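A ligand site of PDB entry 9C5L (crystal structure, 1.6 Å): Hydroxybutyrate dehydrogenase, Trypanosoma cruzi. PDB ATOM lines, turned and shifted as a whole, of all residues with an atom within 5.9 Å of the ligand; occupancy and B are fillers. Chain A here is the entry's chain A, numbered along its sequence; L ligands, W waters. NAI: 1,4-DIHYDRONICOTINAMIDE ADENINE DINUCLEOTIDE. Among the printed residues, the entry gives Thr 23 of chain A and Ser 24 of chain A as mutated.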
ATOM      1  N   THR A  20       5.997   9.994 -16.403  1.00  0.00           N
ATOM      2  CA  THR A  20       6.570   9.275 -17.530  1.00  0.00           C
ATOM      3  C   THR A  20       5.656   8.098 -17.896  1.00  0.00           C
ATOM      4  O   THR A  20       4.982   7.514 -17.048  1.00  0.00           O
ATOM      5  CB  THR A  20       7.983   8.796 -17.209  1.00  0.00           C
ATOM      6  OG1 THR A  20       7.958   7.758 -16.224  1.00  0.00           O
ATOM      7  CG2 THR A  20       8.842   9.964 -16.700  1.00  0.00           C
ATOM      8  N   GLY A  21       5.592   7.796 -19.196  1.00  0.00           N
ATOM      9  CA  GLY A  21       4.810   6.685 -19.661  1.00  0.00           C
ATOM     10  C   GLY A  21       3.333   6.804 -19.317  1.00  0.00           C
ATOM     11  O   GLY A  21       2.728   5.876 -18.785  1.00  0.00           O
ATOM     12  N   SER A  22       2.752   7.972 -19.607  1.00  0.00           N
ATOM     13  CA  SER A  22       1.385   8.304 -19.194  1.00  0.00           C
ATOM     14  C   SER A  22       0.415   8.345 -20.379  1.00  0.00           C
ATOM     15  O   SER A  22      -0.646   8.951 -20.256  1.00  0.00           O
ATOM     16  CB  SER A  22       1.349   9.633 -18.444  1.00  0.00           C
ATOM     17  OG  SER A  22       2.178  10.595 -19.084  1.00  0.00           O
ATOM     18  N   THR A  23       0.728   7.660 -21.465  1.00  0.00           N
ATOM     19  CA  THR A  23      -0.190   7.572 -22.593  1.00  0.00           C
ATOM     20  C   THR A  23      -1.110   6.376 -22.509  1.00  0.00           C
ATOM     21  O   THR A  23      -1.982   6.213 -23.387  1.00  0.00           O
ATOM     22  CB  THR A  23       0.597   7.554 -23.912  1.00  0.00           C
ATOM     23  OG1 THR A  23       1.515   6.464 -23.923  1.00  0.00           O
ATOM     24  CG2 THR A  23       1.359   8.855 -24.085  1.00  0.00           C
ATOM     25  N   SER A  24      -0.927   5.516 -21.494  1.00  0.00           N
ATOM     26  CA  SER A  24      -1.673   4.283 -21.362  1.00  0.00           C
ATOM     27  C   SER A  24      -1.694   3.870 -19.896  1.00  0.00           C
ATOM     28  O   SER A  24      -0.861   4.315 -19.099  1.00  0.00           O
ATOM     29  CB  SER A  24      -1.037   3.171 -22.208  1.00  0.00           C
ATOM     30  OG  SER A  24      -1.631   1.912 -21.954  1.00  0.00           O
ATOM     31  N   GLY A  25      -2.667   3.034 -19.562  1.00  0.00           N
ATOM     32  CA  GLY A  25      -2.620   2.243 -18.327  1.00  0.00           C
ATOM     33  C   GLY A  25      -2.434   3.066 -17.057  1.00  0.00           C
ATOM     34  O   GLY A  25      -3.096   4.075 -16.795  1.00  0.00           O
ATOM     35  N   ILE A  26      -1.537   2.578 -16.185  1.00  0.00           N
ATOM     36  CA  ILE A  26      -1.395   3.194 -14.881  1.00  0.00           C
ATOM     37  C   ILE A  26      -0.912   4.635 -14.976  1.00  0.00           C
ATOM     38  O   ILE A  26      -1.381   5.493 -14.249  1.00  0.00           O
ATOM     39  CB  ILE A  26      -0.451   2.334 -14.012  1.00  0.00           C
ATOM     40  CG1 ILE A  26      -1.131   1.070 -13.568  1.00  0.00           C
ATOM     41  CG2 ILE A  26       0.056   3.166 -12.838  1.00  0.00           C
ATOM     42  CD1 ILE A  26      -0.200   0.035 -12.985  1.00  0.00           C
ATOM     43  N   GLY A  27       0.033   4.914 -15.879  1.00  0.00           N
ATOM     44  CA  GLY A  27       0.524   6.283 -16.012  1.00  0.00           C
ATOM     45  C   GLY A  27      -0.569   7.271 -16.378  1.00  0.00           C
ATOM     46  O   GLY A  27      -0.637   8.375 -15.825  1.00  0.00           O
ATOM     47  N   ASN A  44       3.705  11.845 -21.282  1.00  0.00           N
ATOM     48  CA  ASN A  44       4.857  11.339 -22.024  1.00  0.00           C
ATOM     49  C   ASN A  44       4.596   9.926 -22.525  1.00  0.00           C
ATOM     50  O   ASN A  44       4.027   9.107 -21.808  1.00  0.00           O
ATOM     51  CB  ASN A  44       6.106  11.353 -21.117  1.00  0.00           C
ATOM     52  CG  ASN A  44       7.196  10.402 -21.602  1.00  0.00           C
ATOM     53  OD1 ASN A  44       7.353   9.287 -21.082  1.00  0.00           O
ATOM     54  ND2 ASN A  44       7.954  10.830 -22.609  1.00  0.00           N
ATOM     55  N   GLY A  45       5.018   9.674 -23.761  1.00  0.00           N
ATOM     56  CA  GLY A  45       5.088   8.322 -24.277  1.00  0.00           C
ATOM     57  C   GLY A  45       6.377   8.148 -25.051  1.00  0.00           C
ATOM     58  O   GLY A  45       7.076   9.112 -25.332  1.00  0.00           O
ATOM     59  N   ARG A  46       6.664   6.891 -25.382  1.00  0.00           N
ATOM     60  CA  ARG A  46       7.914   6.568 -26.053  1.00  0.00           C
ATOM     61  C   ARG A  46       8.053   7.315 -27.360  1.00  0.00           C
ATOM     62  O   ARG A  46       9.114   7.859 -27.671  1.00  0.00           O
ATOM     63  CB  ARG A  46       7.986   5.051 -26.264  1.00  0.00           C
ATOM     64  CG  ARG A  46       9.028   4.554 -27.231  1.00  0.00           C
ATOM     65  CD  ARG A  46      10.441   4.868 -26.783  1.00  0.00           C
ATOM     66  NE  ARG A  46      11.443   4.314 -27.694  1.00  0.00           N
ATOM     67  CZ  ARG A  46      11.909   4.937 -28.766  1.00  0.00           C
ATOM     68  NH1 ARG A  46      11.522   6.170 -29.073  1.00  0.00           N
ATOM     69  NH2 ARG A  46      12.795   4.327 -29.542  1.00  0.00           N
ATOM     70  N   ALA A  71       9.275  11.136 -25.616  1.00  0.00           N
ATOM     71  CA  ALA A  71      10.667  10.966 -25.244  1.00  0.00           C
ATOM     72  C   ALA A  71      10.899   9.538 -24.788  1.00  0.00           C
ATOM     73  O   ALA A  71      10.090   8.986 -24.040  1.00  0.00           O
ATOM     74  CB  ALA A  71      11.081  11.942 -24.140  1.00  0.00           C
ATOM     75  N   ASN A  72      11.996   8.954 -25.257  1.00  0.00           N
ATOM     76  CA  ASN A  72      12.405   7.604 -24.873  1.00  0.00           C
ATOM     77  C   ASN A  72      13.172   7.696 -23.562  1.00  0.00           C
ATOM     78  O   ASN A  72      14.296   8.188 -23.528  1.00  0.00           O
ATOM     79  CB  ASN A  72      13.267   6.993 -25.971  1.00  0.00           C
ATOM     80  CG  ASN A  72      13.839   5.653 -25.594  1.00  0.00           C
ATOM     81  OD1 ASN A  72      13.447   5.057 -24.582  1.00  0.00           O
ATOM     82  ND2 ASN A  72      14.775   5.159 -26.410  1.00  0.00           N
ATOM     83  N   MET A  73      12.556   7.196 -22.475  1.00  0.00           N
ATOM     84  CA  MET A  73      13.156   7.315 -21.150  1.00  0.00           C
ATOM     85  C   MET A  73      14.425   6.480 -20.975  1.00  0.00           C
ATOM     86  O   MET A  73      15.136   6.663 -19.987  1.00  0.00           O
ATOM     87  CB  MET A  73      12.133   6.933 -20.076  1.00  0.00           C
ATOM     88  CG  MET A  73      10.934   7.868 -19.962  1.00  0.00           C
ATOM     89  SD  MET A  73      11.342   9.554 -19.498  1.00  0.00           S
ATOM     90  CE  MET A  73      11.583  10.363 -21.071  1.00  0.00           C
ATOM     91  N   LYS A  74      14.736   5.598 -21.923  1.00  0.00           N
ATOM     92  CA  LYS A  74      16.001   4.879 -21.900  1.00  0.00           C
ATOM     93  C   LYS A  74      17.164   5.737 -22.389  1.00  0.00           C
ATOM     94  O   LYS A  74      18.311   5.286 -22.298  1.00  0.00           O
ATOM     95  CB  LYS A  74      15.904   3.605 -22.743  1.00  0.00           C
ATOM     96  CG  LYS A  74      14.895   2.586 -22.173  1.00  0.00           C
ATOM     97  CD  LYS A  74      14.861   1.292 -22.981  1.00  0.00           C
ATOM     98  CE  LYS A  74      14.165   1.483 -24.314  1.00  0.00           C
ATOM     99  NZ  LYS A  74      13.989   0.182 -25.044  1.00  0.00           N
ATOM    100  N   ASN A  98       7.836   8.534 -11.724  1.00  0.00           N
ATOM    101  CA  ASN A  98       8.600   7.619 -12.562  1.00  0.00           C
ATOM    102  C   ASN A  98       7.757   6.378 -12.748  1.00  0.00           C
ATOM    103  O   ASN A  98       7.639   5.547 -11.837  1.00  0.00           O
ATOM    104  CB  ASN A  98       9.939   7.301 -11.926  1.00  0.00           C
ATOM    105  CG  ASN A  98      10.888   8.484 -11.914  1.00  0.00           C
ATOM    106  OD1 ASN A  98      11.155   9.085 -12.950  1.00  0.00           O
ATOM    107  ND2 ASN A  98      11.401   8.836 -10.736  1.00  0.00           N
ATOM    108  N   ASN A  99       7.161   6.247 -13.935  1.00  0.00           N
ATOM    109  CA  ASN A  99       6.158   5.198 -14.130  1.00  0.00           C
ATOM    110  C   ASN A  99       6.451   4.310 -15.327  1.00  0.00           C
ATOM    111  O   ASN A  99       6.088   3.127 -15.321  1.00  0.00           O
ATOM    112  CB  ASN A  99       4.765   5.804 -14.283  1.00  0.00           C
ATOM    113  CG  ASN A  99       3.733   4.815 -14.813  1.00  0.00           C
ATOM    114  OD1 ASN A  99       3.151   4.040 -14.046  1.00  0.00           O
ATOM    115  ND2 ASN A  99       3.487   4.829 -16.124  1.00  0.00           N
ATOM    116  N   ALA A 100       7.030   4.875 -16.378  1.00  0.00           N
ATOM    117  CA  ALA A 100       7.202   4.088 -17.600  1.00  0.00           C
ATOM    118  C   ALA A 100       7.860   2.754 -17.249  1.00  0.00           C
ATOM    119  O   ALA A 100       8.867   2.699 -16.527  1.00  0.00           O
ATOM    120  CB  ALA A 100       8.040   4.874 -18.630  1.00  0.00           C
ATOM    121  N   GLY A 101       7.274   1.662 -17.735  1.00  0.00           N
ATOM    122  CA  GLY A 101       7.768   0.346 -17.420  1.00  0.00           C
ATOM    123  C   GLY A 101       7.371  -0.649 -18.482  1.00  0.00           C
ATOM    124  O   GLY A 101       6.409  -0.436 -19.225  1.00  0.00           O
ATOM    125  N   ILE A 102       8.126  -1.762 -18.520  1.00  0.00           N
ATOM    126  CA  ILE A 102       7.893  -2.857 -19.449  1.00  0.00           C
ATOM    127  C   ILE A 102       8.071  -4.183 -18.703  1.00  0.00           C
ATOM    128  O   ILE A 102       8.702  -4.250 -17.643  1.00  0.00           O
ATOM    129  CB  ILE A 102       8.840  -2.839 -20.653  1.00  0.00           C
ATOM    130  CG1 ILE A 102      10.286  -2.772 -20.178  1.00  0.00           C
ATOM    131  CG2 ILE A 102       8.513  -1.631 -21.577  1.00  0.00           C
ATOM    132  CD1 ILE A 102      11.293  -2.858 -21.312  1.00  0.00           C
ATOM    133  N   LEU A 122      14.860   0.608 -18.163  1.00  0.00           N
ATOM    134  CA  LEU A 122      13.664   1.441 -18.114  1.00  0.00           C
ATOM    135  C   LEU A 122      13.036   1.442 -16.729  1.00  0.00           C
ATOM    136  O   LEU A 122      12.660   2.502 -16.220  1.00  0.00           O
ATOM    137  CB  LEU A 122      12.635   0.986 -19.144  1.00  0.00           C
ATOM    138  CG  LEU A 122      11.344   1.789 -19.107  1.00  0.00           C
ATOM    139  CD1 LEU A 122      11.571   3.274 -19.468  1.00  0.00           C
ATOM    140  CD2 LEU A 122      10.307   1.187 -20.044  1.00  0.00           C
ATOM    141  N   ASN A 123      12.928   0.257 -16.101  1.00  0.00           N
ATOM    142  CA  ASN A 123      12.173   0.180 -14.869  1.00  0.00           C
ATOM    143  C   ASN A 123      12.986   0.643 -13.646  1.00  0.00           C
ATOM    144  O   ASN A 123      12.384   0.855 -12.573  1.00  0.00           O
ATOM    145  CB  ASN A 123      11.699  -1.260 -14.656  1.00  0.00           C
ATOM    146  CG  ASN A 123      10.770  -1.753 -15.761  1.00  0.00           C
ATOM    147  OD1 ASN A 123      10.663  -1.143 -16.820  1.00  0.00           O
ATOM    148  ND2 ASN A 123      10.130  -2.881 -15.532  1.00  0.00           N
ATOM    149  N   ILE A 149       6.743   4.316  -9.358  1.00  0.00           N
ATOM    150  CA  ILE A 149       5.772   3.243  -9.545  1.00  0.00           C
ATOM    151  C   ILE A 149       6.576   1.950  -9.598  1.00  0.00           C
ATOM    152  O   ILE A 149       7.164   1.599 -10.615  1.00  0.00           O
ATOM    153  CB  ILE A 149       4.904   3.450 -10.783  1.00  0.00           C
ATOM    154  CG1 ILE A 149       4.276   4.866 -10.774  1.00  0.00           C
ATOM    155  CG2 ILE A 149       3.824   2.343 -10.858  1.00  0.00           C
ATOM    156  CD1 ILE A 149       3.522   5.194  -9.481  1.00  0.00           C
ATOM    157  N   ALA A 150       6.606   1.264  -8.466  1.00  0.00           N
ATOM    158  CA  ALA A 150       7.192  -0.051  -8.269  1.00  0.00           C
ATOM    159  C   ALA A 150       6.102  -1.086  -8.555  1.00  0.00           C
ATOM    160  O   ALA A 150       5.413  -0.992  -9.605  1.00  0.00           O
ATOM    161  CB  ALA A 150       7.816  -0.147  -6.895  1.00  0.00           C
ATOM    162  N   SER A 151       6.067  -2.148  -7.772  1.00  0.00           N
ATOM    163  CA  SER A 151       5.132  -3.253  -7.939  1.00  0.00           C
ATOM    164  C   SER A 151       5.218  -4.107  -6.679  1.00  0.00           C
ATOM    165  O   SER A 151       6.173  -4.003  -5.909  1.00  0.00           O
ATOM    166  CB  SER A 151       5.503  -4.107  -9.176  1.00  0.00           C
ATOM    167  OG  SER A 151       4.746  -5.292  -9.262  1.00  0.00           O
ATOM    168  N   VAL A 152       4.181  -4.914  -6.470  1.00  0.00           N
ATOM    169  CA  VAL A 152       4.321  -6.046  -5.556  1.00  0.00           C
ATOM    170  C   VAL A 152       5.562  -6.846  -5.861  1.00  0.00           C
ATOM    171  O   VAL A 152       6.203  -7.414  -4.960  1.00  0.00           O
ATOM    172  CB  VAL A 152       3.085  -6.964  -5.591  1.00  0.00           C
ATOM    173  CG1 VAL A 152       1.874  -6.243  -4.998  1.00  0.00           C
ATOM    174  CG2 VAL A 152       2.800  -7.491  -6.990  1.00  0.00           C
ATOM    175  N   TYR A 164      12.170  -8.252 -14.092  1.00  0.00           N
ATOM    176  CA  TYR A 164      11.197  -7.288 -13.569  1.00  0.00           C
ATOM    177  C   TYR A 164      11.203  -7.244 -12.037  1.00  0.00           C
ATOM    178  O   TYR A 164      11.235  -6.157 -11.452  1.00  0.00           O
ATOM    179  CB  TYR A 164       9.839  -7.669 -14.105  1.00  0.00           C
ATOM    180  CG  TYR A 164       8.699  -6.738 -13.831  1.00  0.00           C
ATOM    181  CD1 TYR A 164       8.329  -5.766 -14.739  1.00  0.00           C
ATOM    182  CD2 TYR A 164       7.927  -6.893 -12.693  1.00  0.00           C
ATOM    183  CE1 TYR A 164       7.252  -4.950 -14.507  1.00  0.00           C
ATOM    184  CE2 TYR A 164       6.834  -6.084 -12.459  1.00  0.00           C
ATOM    185  CZ  TYR A 164       6.499  -5.119 -13.367  1.00  0.00           C
ATOM    186  OH  TYR A 164       5.409  -4.331 -13.155  1.00  0.00           O
ATOM    187  N   LYS A 168      12.250  -3.906  -9.969  1.00  0.00           N
ATOM    188  CA  LYS A 168      11.290  -3.281  -9.081  1.00  0.00           C
ATOM    189  C   LYS A 168      11.815  -3.275  -7.636  1.00  0.00           C
ATOM    190  O   LYS A 168      11.574  -2.305  -6.901  1.00  0.00           O
ATOM    191  CB  LYS A 168       9.930  -3.953  -9.189  1.00  0.00           C
ATOM    192  CG  LYS A 168       9.221  -3.760 -10.525  1.00  0.00           C
ATOM    193  CD  LYS A 168       8.899  -2.293 -10.788  1.00  0.00           C
ATOM    194  CE  LYS A 168       7.913  -2.156 -11.986  1.00  0.00           C
ATOM    195  NZ  LYS A 168       7.704  -0.742 -12.355  1.00  0.00           N
ATOM    196  N   CYS A 193       3.219   0.448  -4.896  1.00  0.00           N
ATOM    197  CA  CYS A 193       3.409  -0.945  -5.287  1.00  0.00           C
ATOM    198  C   CYS A 193       2.065  -1.575  -5.644  1.00  0.00           C
ATOM    199  O   CYS A 193       1.392  -2.184  -4.777  1.00  0.00           O
ATOM    200  CB  CYS A 193       4.075  -1.759  -4.191  1.00  0.00           C
ATOM    201  SG  CYS A 193       5.753  -1.239  -3.784  1.00  0.00           S
ATOM    202  N   PRO A 194       1.615  -1.416  -6.881  1.00  0.00           N
ATOM    203  CA  PRO A 194       0.356  -2.069  -7.307  1.00  0.00           C
ATOM    204  C   PRO A 194       0.534  -3.563  -7.462  1.00  0.00           C
ATOM    205  O   PRO A 194       1.618  -4.058  -7.792  1.00  0.00           O
ATOM    206  CB  PRO A 194       0.041  -1.421  -8.651  1.00  0.00           C
ATOM    207  CG  PRO A 194       0.944  -0.217  -8.750  1.00  0.00           C
ATOM    208  CD  PRO A 194       2.175  -0.552  -7.931  1.00  0.00           C
ATOM    209  N   GLY A 195      -0.559  -4.277  -7.185  1.00  0.00           N
ATOM    210  CA  GLY A 195      -0.745  -5.643  -7.639  1.00  0.00           C
ATOM    211  C   GLY A 195      -1.237  -5.595  -9.070  1.00  0.00           C
ATOM    212  O   GLY A 195      -0.983  -4.636  -9.810  1.00  0.00           O
ATOM    213  N   TYR A 196      -1.993  -6.612  -9.477  1.00  0.00           N
ATOM    214  CA  TYR A 196      -2.493  -6.638 -10.847  1.00  0.00           C
ATOM    215  C   TYR A 196      -3.525  -5.558 -11.116  1.00  0.00           C
ATOM    216  O   TYR A 196      -4.533  -5.461 -10.400  1.00  0.00           O
ATOM    217  CB  TYR A 196      -3.107  -7.985 -11.135  1.00  0.00           C
ATOM    218  CG  TYR A 196      -2.136  -9.139 -11.281  1.00  0.00           C
ATOM    219  CD1 TYR A 196      -0.895  -8.968 -11.868  1.00  0.00           C
ATOM    220  CD2 TYR A 196      -2.513 -10.448 -10.881  1.00  0.00           C
ATOM    221  CE1 TYR A 196      -0.041 -10.047 -12.075  1.00  0.00           C
ATOM    222  CE2 TYR A 196      -1.657 -11.490 -11.049  1.00  0.00           C
ATOM    223  CZ  TYR A 196      -0.418 -11.274 -11.632  1.00  0.00           C
ATOM    224  OH  TYR A 196       0.413 -12.382 -11.815  1.00  0.00           O
ATOM    225  N   VAL A 197      -3.303  -4.808 -12.208  1.00  0.00           N
ATOM    226  CA  VAL A 197      -4.162  -3.758 -12.746  1.00  0.00           C
ATOM    227  C   VAL A 197      -4.443  -4.117 -14.215  1.00  0.00           C
ATOM    228  O   VAL A 197      -3.544  -4.567 -14.940  1.00  0.00           O
ATOM    229  CB  VAL A 197      -3.464  -2.384 -12.626  1.00  0.00           C
ATOM    230  CG1 VAL A 197      -4.407  -1.278 -13.117  1.00  0.00           C
ATOM    231  CG2 VAL A 197      -2.996  -2.124 -11.230  1.00  0.00           C
ATOM    232  N   TYR A 198      -5.681  -3.951 -14.660  1.00  0.00           N
ATOM    233  CA  TYR A 198      -6.003  -4.438 -16.004  1.00  0.00           C
ATOM    234  C   TYR A 198      -5.642  -3.364 -17.038  1.00  0.00           C
ATOM    235  O   TYR A 198      -6.490  -2.678 -17.605  1.00  0.00           O
ATOM    236  CB  TYR A 198      -7.463  -4.856 -16.128  1.00  0.00           C
ATOM    237  CG  TYR A 198      -7.737  -5.745 -17.331  1.00  0.00           C
ATOM    238  CD1 TYR A 198      -7.333  -7.072 -17.339  1.00  0.00           C
ATOM    239  CD2 TYR A 198      -8.422  -5.271 -18.441  1.00  0.00           C
ATOM    240  CE1 TYR A 198      -7.624  -7.917 -18.439  1.00  0.00           C
ATOM    241  CE2 TYR A 198      -8.681  -6.077 -19.536  1.00  0.00           C
ATOM    242  CZ  TYR A 198      -8.262  -7.408 -19.517  1.00  0.00           C
ATOM    243  OH  TYR A 198      -8.535  -8.237 -20.597  1.00  0.00           O
ATOM    244  N   THR A 199      -4.363  -3.286 -17.314  1.00  0.00           N
ATOM    245  CA  THR A 199      -3.778  -2.458 -18.360  1.00  0.00           C
ATOM    246  C   THR A 199      -3.401  -3.320 -19.561  1.00  0.00           C
ATOM    247  O   THR A 199      -3.485  -4.544 -19.520  1.00  0.00           O
ATOM    248  CB  THR A 199      -2.539  -1.785 -17.838  1.00  0.00           C
ATOM    249  OG1 THR A 199      -1.532  -2.799 -17.718  1.00  0.00           O
ATOM    250  CG2 THR A 199      -2.809  -1.129 -16.498  1.00  0.00           C
ATOM    251  N   PRO A 200      -2.980  -2.700 -20.663  1.00  0.00           N
ATOM    252  CA  PRO A 200      -2.435  -3.506 -21.773  1.00  0.00           C
ATOM    253  C   PRO A 200      -1.229  -4.354 -21.386  1.00  0.00           C
ATOM    254  O   PRO A 200      -1.098  -5.479 -21.902  1.00  0.00           O
ATOM    255  CB  PRO A 200      -2.073  -2.447 -22.817  1.00  0.00           C
ATOM    256  CG  PRO A 200      -3.045  -1.321 -22.550  1.00  0.00           C
ATOM    257  CD  PRO A 200      -3.186  -1.292 -21.045  1.00  0.00           C
ATOM    258  N   LEU A 201      -0.367  -3.882 -20.478  1.00  0.00           N
ATOM    259  CA  LEU A 201       0.743  -4.700 -20.003  1.00  0.00           C
ATOM    260  C   LEU A 201       0.254  -6.014 -19.395  1.00  0.00           C
ATOM    261  O   LEU A 201       0.902  -7.064 -19.549  1.00  0.00           O
ATOM    262  CB  LEU A 201       1.564  -3.903 -18.984  1.00  0.00           C
ATOM    263  CG  LEU A 201       2.811  -4.543 -18.351  1.00  0.00           C
ATOM    264  CD1 LEU A 201       3.864  -3.485 -18.081  1.00  0.00           C
ATOM    265  CD2 LEU A 201       2.481  -5.320 -17.049  1.00  0.00           C
ATOM    266  N   VAL A 202      -0.898  -5.983 -18.723  1.00  0.00           N
ATOM    267  CA  VAL A 202      -1.437  -7.181 -18.095  1.00  0.00           C
ATOM    268  C   VAL A 202      -2.364  -7.927 -19.037  1.00  0.00           C
ATOM    269  O   VAL A 202      -2.361  -9.163 -19.069  1.00  0.00           O
ATOM    270  CB  VAL A 202      -2.163  -6.792 -16.800  1.00  0.00           C
ATOM    271  CG1 VAL A 202      -3.116  -7.882 -16.353  1.00  0.00           C
ATOM    272  CG2 VAL A 202      -1.122  -6.523 -15.680  1.00  0.00           C
HETATM  273  PA  NAI L   1       1.243   0.062 -20.089  1.00  0.00           P
HETATM  274  O1A NAI L   1       1.944  -0.739 -21.111  1.00  0.00           O
HETATM  275  O2A NAI L   1      -0.267   0.231 -20.162  1.00  0.00           O
HETATM  276  O5B NAI L   1       1.894   1.517 -19.981  1.00  0.00           O
HETATM  277  C5B NAI L   1       3.306   1.708 -20.181  1.00  0.00           C
HETATM  278  C4B NAI L   1       3.545   3.175 -20.470  1.00  0.00           C
HETATM  279  O4B NAI L   1       4.972   3.330 -20.558  1.00  0.00           O
HETATM  280  C3B NAI L   1       2.995   3.537 -21.851  1.00  0.00           C
HETATM  281  O3B NAI L   1       2.695   4.929 -21.821  1.00  0.00           O
HETATM  282  C2B NAI L   1       4.232   3.395 -22.734  1.00  0.00           C
HETATM  283  O2B NAI L   1       4.131   4.347 -23.781  1.00  0.00           O
HETATM  284  C1B NAI L   1       5.276   3.959 -21.779  1.00  0.00           C
HETATM  285  N9A NAI L   1       6.636   3.565 -22.158  1.00  0.00           N
HETATM  286  C8A NAI L   1       7.106   2.306 -22.433  1.00  0.00           C
HETATM  287  N7A NAI L   1       8.373   2.274 -22.773  1.00  0.00           N
HETATM  288  C5A NAI L   1       8.757   3.612 -22.732  1.00  0.00           C
HETATM  289  C6A NAI L   1       9.985   4.264 -22.990  1.00  0.00           C
HETATM  290  N6A NAI L   1      11.091   3.627 -23.364  1.00  0.00           N
HETATM  291  N1A NAI L   1      10.020   5.622 -22.879  1.00  0.00           N
HETATM  292  C2A NAI L   1       8.906   6.263 -22.500  1.00  0.00           C
HETATM  293  N3A NAI L   1       7.703   5.756 -22.221  1.00  0.00           N
HETATM  294  C4A NAI L   1       7.689   4.418 -22.353  1.00  0.00           C
HETATM  295  O3  NAI L   1       1.636  -0.501 -18.658  1.00  0.00           O
HETATM  296  PN  NAI L   1       1.193  -0.254 -17.166  1.00  0.00           P
HETATM  297  O1N NAI L   1       0.290   0.954 -17.070  1.00  0.00           O
HETATM  298  O2N NAI L   1       0.598  -1.578 -16.580  1.00  0.00           O
HETATM  299  O5D NAI L   1       2.551   0.008 -16.463  1.00  0.00           O
HETATM  300  C5D NAI L   1       2.845   1.283 -15.850  1.00  0.00           C
HETATM  301  C4D NAI L   1       3.782   1.007 -14.695  1.00  0.00           C
HETATM  302  O4D NAI L   1       3.038   0.288 -13.701  1.00  0.00           O
HETATM  303  C3D NAI L   1       4.925   0.084 -15.113  1.00  0.00           C
HETATM  304  O3D NAI L   1       6.066   0.553 -14.380  1.00  0.00           O
HETATM  305  C2D NAI L   1       4.529  -1.263 -14.513  1.00  0.00           C
HETATM  306  O2D NAI L   1       5.727  -1.883 -14.076  1.00  0.00           O
HETATM  307  C1D NAI L   1       3.840  -0.781 -13.243  1.00  0.00           C
HETATM  308  N1N NAI L   1       2.977  -1.781 -12.632  1.00  0.00           N
HETATM  309  C2N NAI L   1       1.964  -2.378 -13.350  1.00  0.00           C
HETATM  310  C3N NAI L   1       1.173  -3.331 -12.778  1.00  0.00           C
HETATM  311  C7N NAI L   1       0.090  -3.908 -13.563  1.00  0.00           C
HETATM  312  O7N NAI L   1      -0.552  -4.899 -13.127  1.00  0.00           O
HETATM  313  N7N NAI L   1      -0.239  -3.325 -14.718  1.00  0.00           N
HETATM  314  C4N NAI L   1       1.273  -3.652 -11.322  1.00  0.00           C
HETATM  315  C5N NAI L   1       2.479  -3.051 -10.720  1.00  0.00           C
HETATM  316  C6N NAI L   1       3.204  -2.135 -11.335  1.00  0.00           C
HETATM  317  O   HOH W   1      10.431   0.680 -24.160  1.00  0.00           O
HETATM  318  O   HOH W   2       4.756  -1.618 -21.083  1.00  0.00           O
HETATM  319  O   HOH W   3       1.494   3.372 -17.768  1.00  0.00           O
HETATM  320  O   HOH W   4       5.169  -0.220 -23.407  1.00  0.00           O
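N of Val 152 lies within hydrogen-bond range of O of Pro 194, at 3.0 Å.
The backbone carbonyl oxygen (O) of Asn 98 lies within hydrogen-bond range of the backbone NH (N) of Ile 149 (2.9 Å).
The side-chain hydroxyl (OG1) of Thr 20 sits at hydrogen-bond distance from the backbone NH (N) of Ala 100 (3.0 Å).
The backbone NH (N) of Asn 99 sits at hydrogen-bond distance from the side-chain hydroxyl (OG1) of Thr 20 (2.9 Å).
The side-chain amide nitrogen of Asn 99 lies close to the backbone NH of Gly 27 (3.5 Å).
The side-chain hydroxyl (OG1) of Thr 199 is in hydrogen-bond range of the backbone NH (N) of Leu 201 (3.2 Å).
The backbone NH of Lys 74 lies within hydrogen-bond range of the side-chain amide oxygen of Asn 72, 3.0 Å away.
The backbone carbonyl oxygen of Ser 151 is in hydrogen-bond range of the side-chain sulfur of Cys 193 (3.5 Å).
O of Asn 99 sits at hydrogen-bond distance from O3D of the ligand, at 2.7 Å.
N of Thr 23 sits at hydrogen-bond distance from O3B of the ligand.
The side-chain hydroxyl (OG1) of Thr 199 sits at hydrogen-bond distance from an oxygen (O2N) of the ligand, at 2.7 Å.
N of Ile 26 lies within hydrogen-bond range of O1N of the ligand (2.6 Å).
A nitrogen (N6A) of the ligand sits at hydrogen-bond distance from the side-chain amide oxygen (OD1) of Asn 72, at 3.0 Å.
OH of Tyr 164 lies within hydrogen-bond range of O2D of the ligand, at 2.6 Å.
The backbone NH of Met 73 lies within hydrogen-bond range of a nitrogen (N1A) of the ligand.
NZ of Lys 168 lies within hydrogen-bond range of O2D of the ligand, at 2.9 Å.
The side-chain hydroxyl (OG) of Ser 24 sits at hydrogen-bond distance from an oxygen (O2A) of the ligand (2.8 Å).
The backbone NH of Val 197 lies within hydrogen-bond range of an oxygen (O7N) of the ligand (2.9 Å).
The backbone carbonyl oxygen (O) of Gly 21 lies within hydrogen-bond range of an oxygen (O3B) of the ligand (3.2 Å).
The side-chain hydroxyl (OG1) of Thr 23 lies within hydrogen-bond range of an oxygen (O3B) of the ligand (2.9 Å).
Water W3 lies within hydrogen-bond range of O1N of the ligand (2.8 Å), N of Gly 27 (2.8 Å), O of Ser 24 (2.9 Å), ND2 of Asn 99 (3.0 Å) and O of Gly 21 (3.0 Å).
Water W2 bridges O of Gly 101 (2.8 Å) and O1A of the ligand (2.9 Å).
The backbone carbonyl oxygen (O) of Gly 195 lies close to an oxygen (O7N) of the ligand, 3.4 Å away.
Merely in contact with the ligand: Ser 22 (3.8 Å), Gly 25 (3.4 Å), Asn 44 (3.7 Å), Gly 45 (3.9 Å), Arg 46 (3.5 Å), Ala 71 (3.3 Å), Lys 74 (3.9 Å), Ala 100 (3.7 Å), Gly 101 (3.5 Å), Leu 122 (3.5 Å), Ile 149 (3.6 Å), Ala 150 (3.0 Å), Ser 151 (3.5 Å), Pro 194 (3.2 Å), Tyr 196 (3.5 Å), Pro 200 (3.4 Å), Leu 201 (3.4 Å) and Val 202 (3.1 Å).
30 residues have an atom within 4 Å of the ligand: Gly 21, Ser 22, Thr 23, Ser 24, Gly 25, Ile 26, Asn 44, Gly 45, Arg 46, Ala 71, Asn 72, Met 73, Lys 74, Asn 99, Ala 100, Gly 101, Leu 122, Ile 149, Ala 150, Ser 151, Tyr 164, Lys 168, Pro 194, Gly 195, Tyr 196, Val 197, Thr 199, Pro 200, Leu 201 and Val 202.
The nearest printed residue that does not touch the ligand is Ile 102 (4.1 Å).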
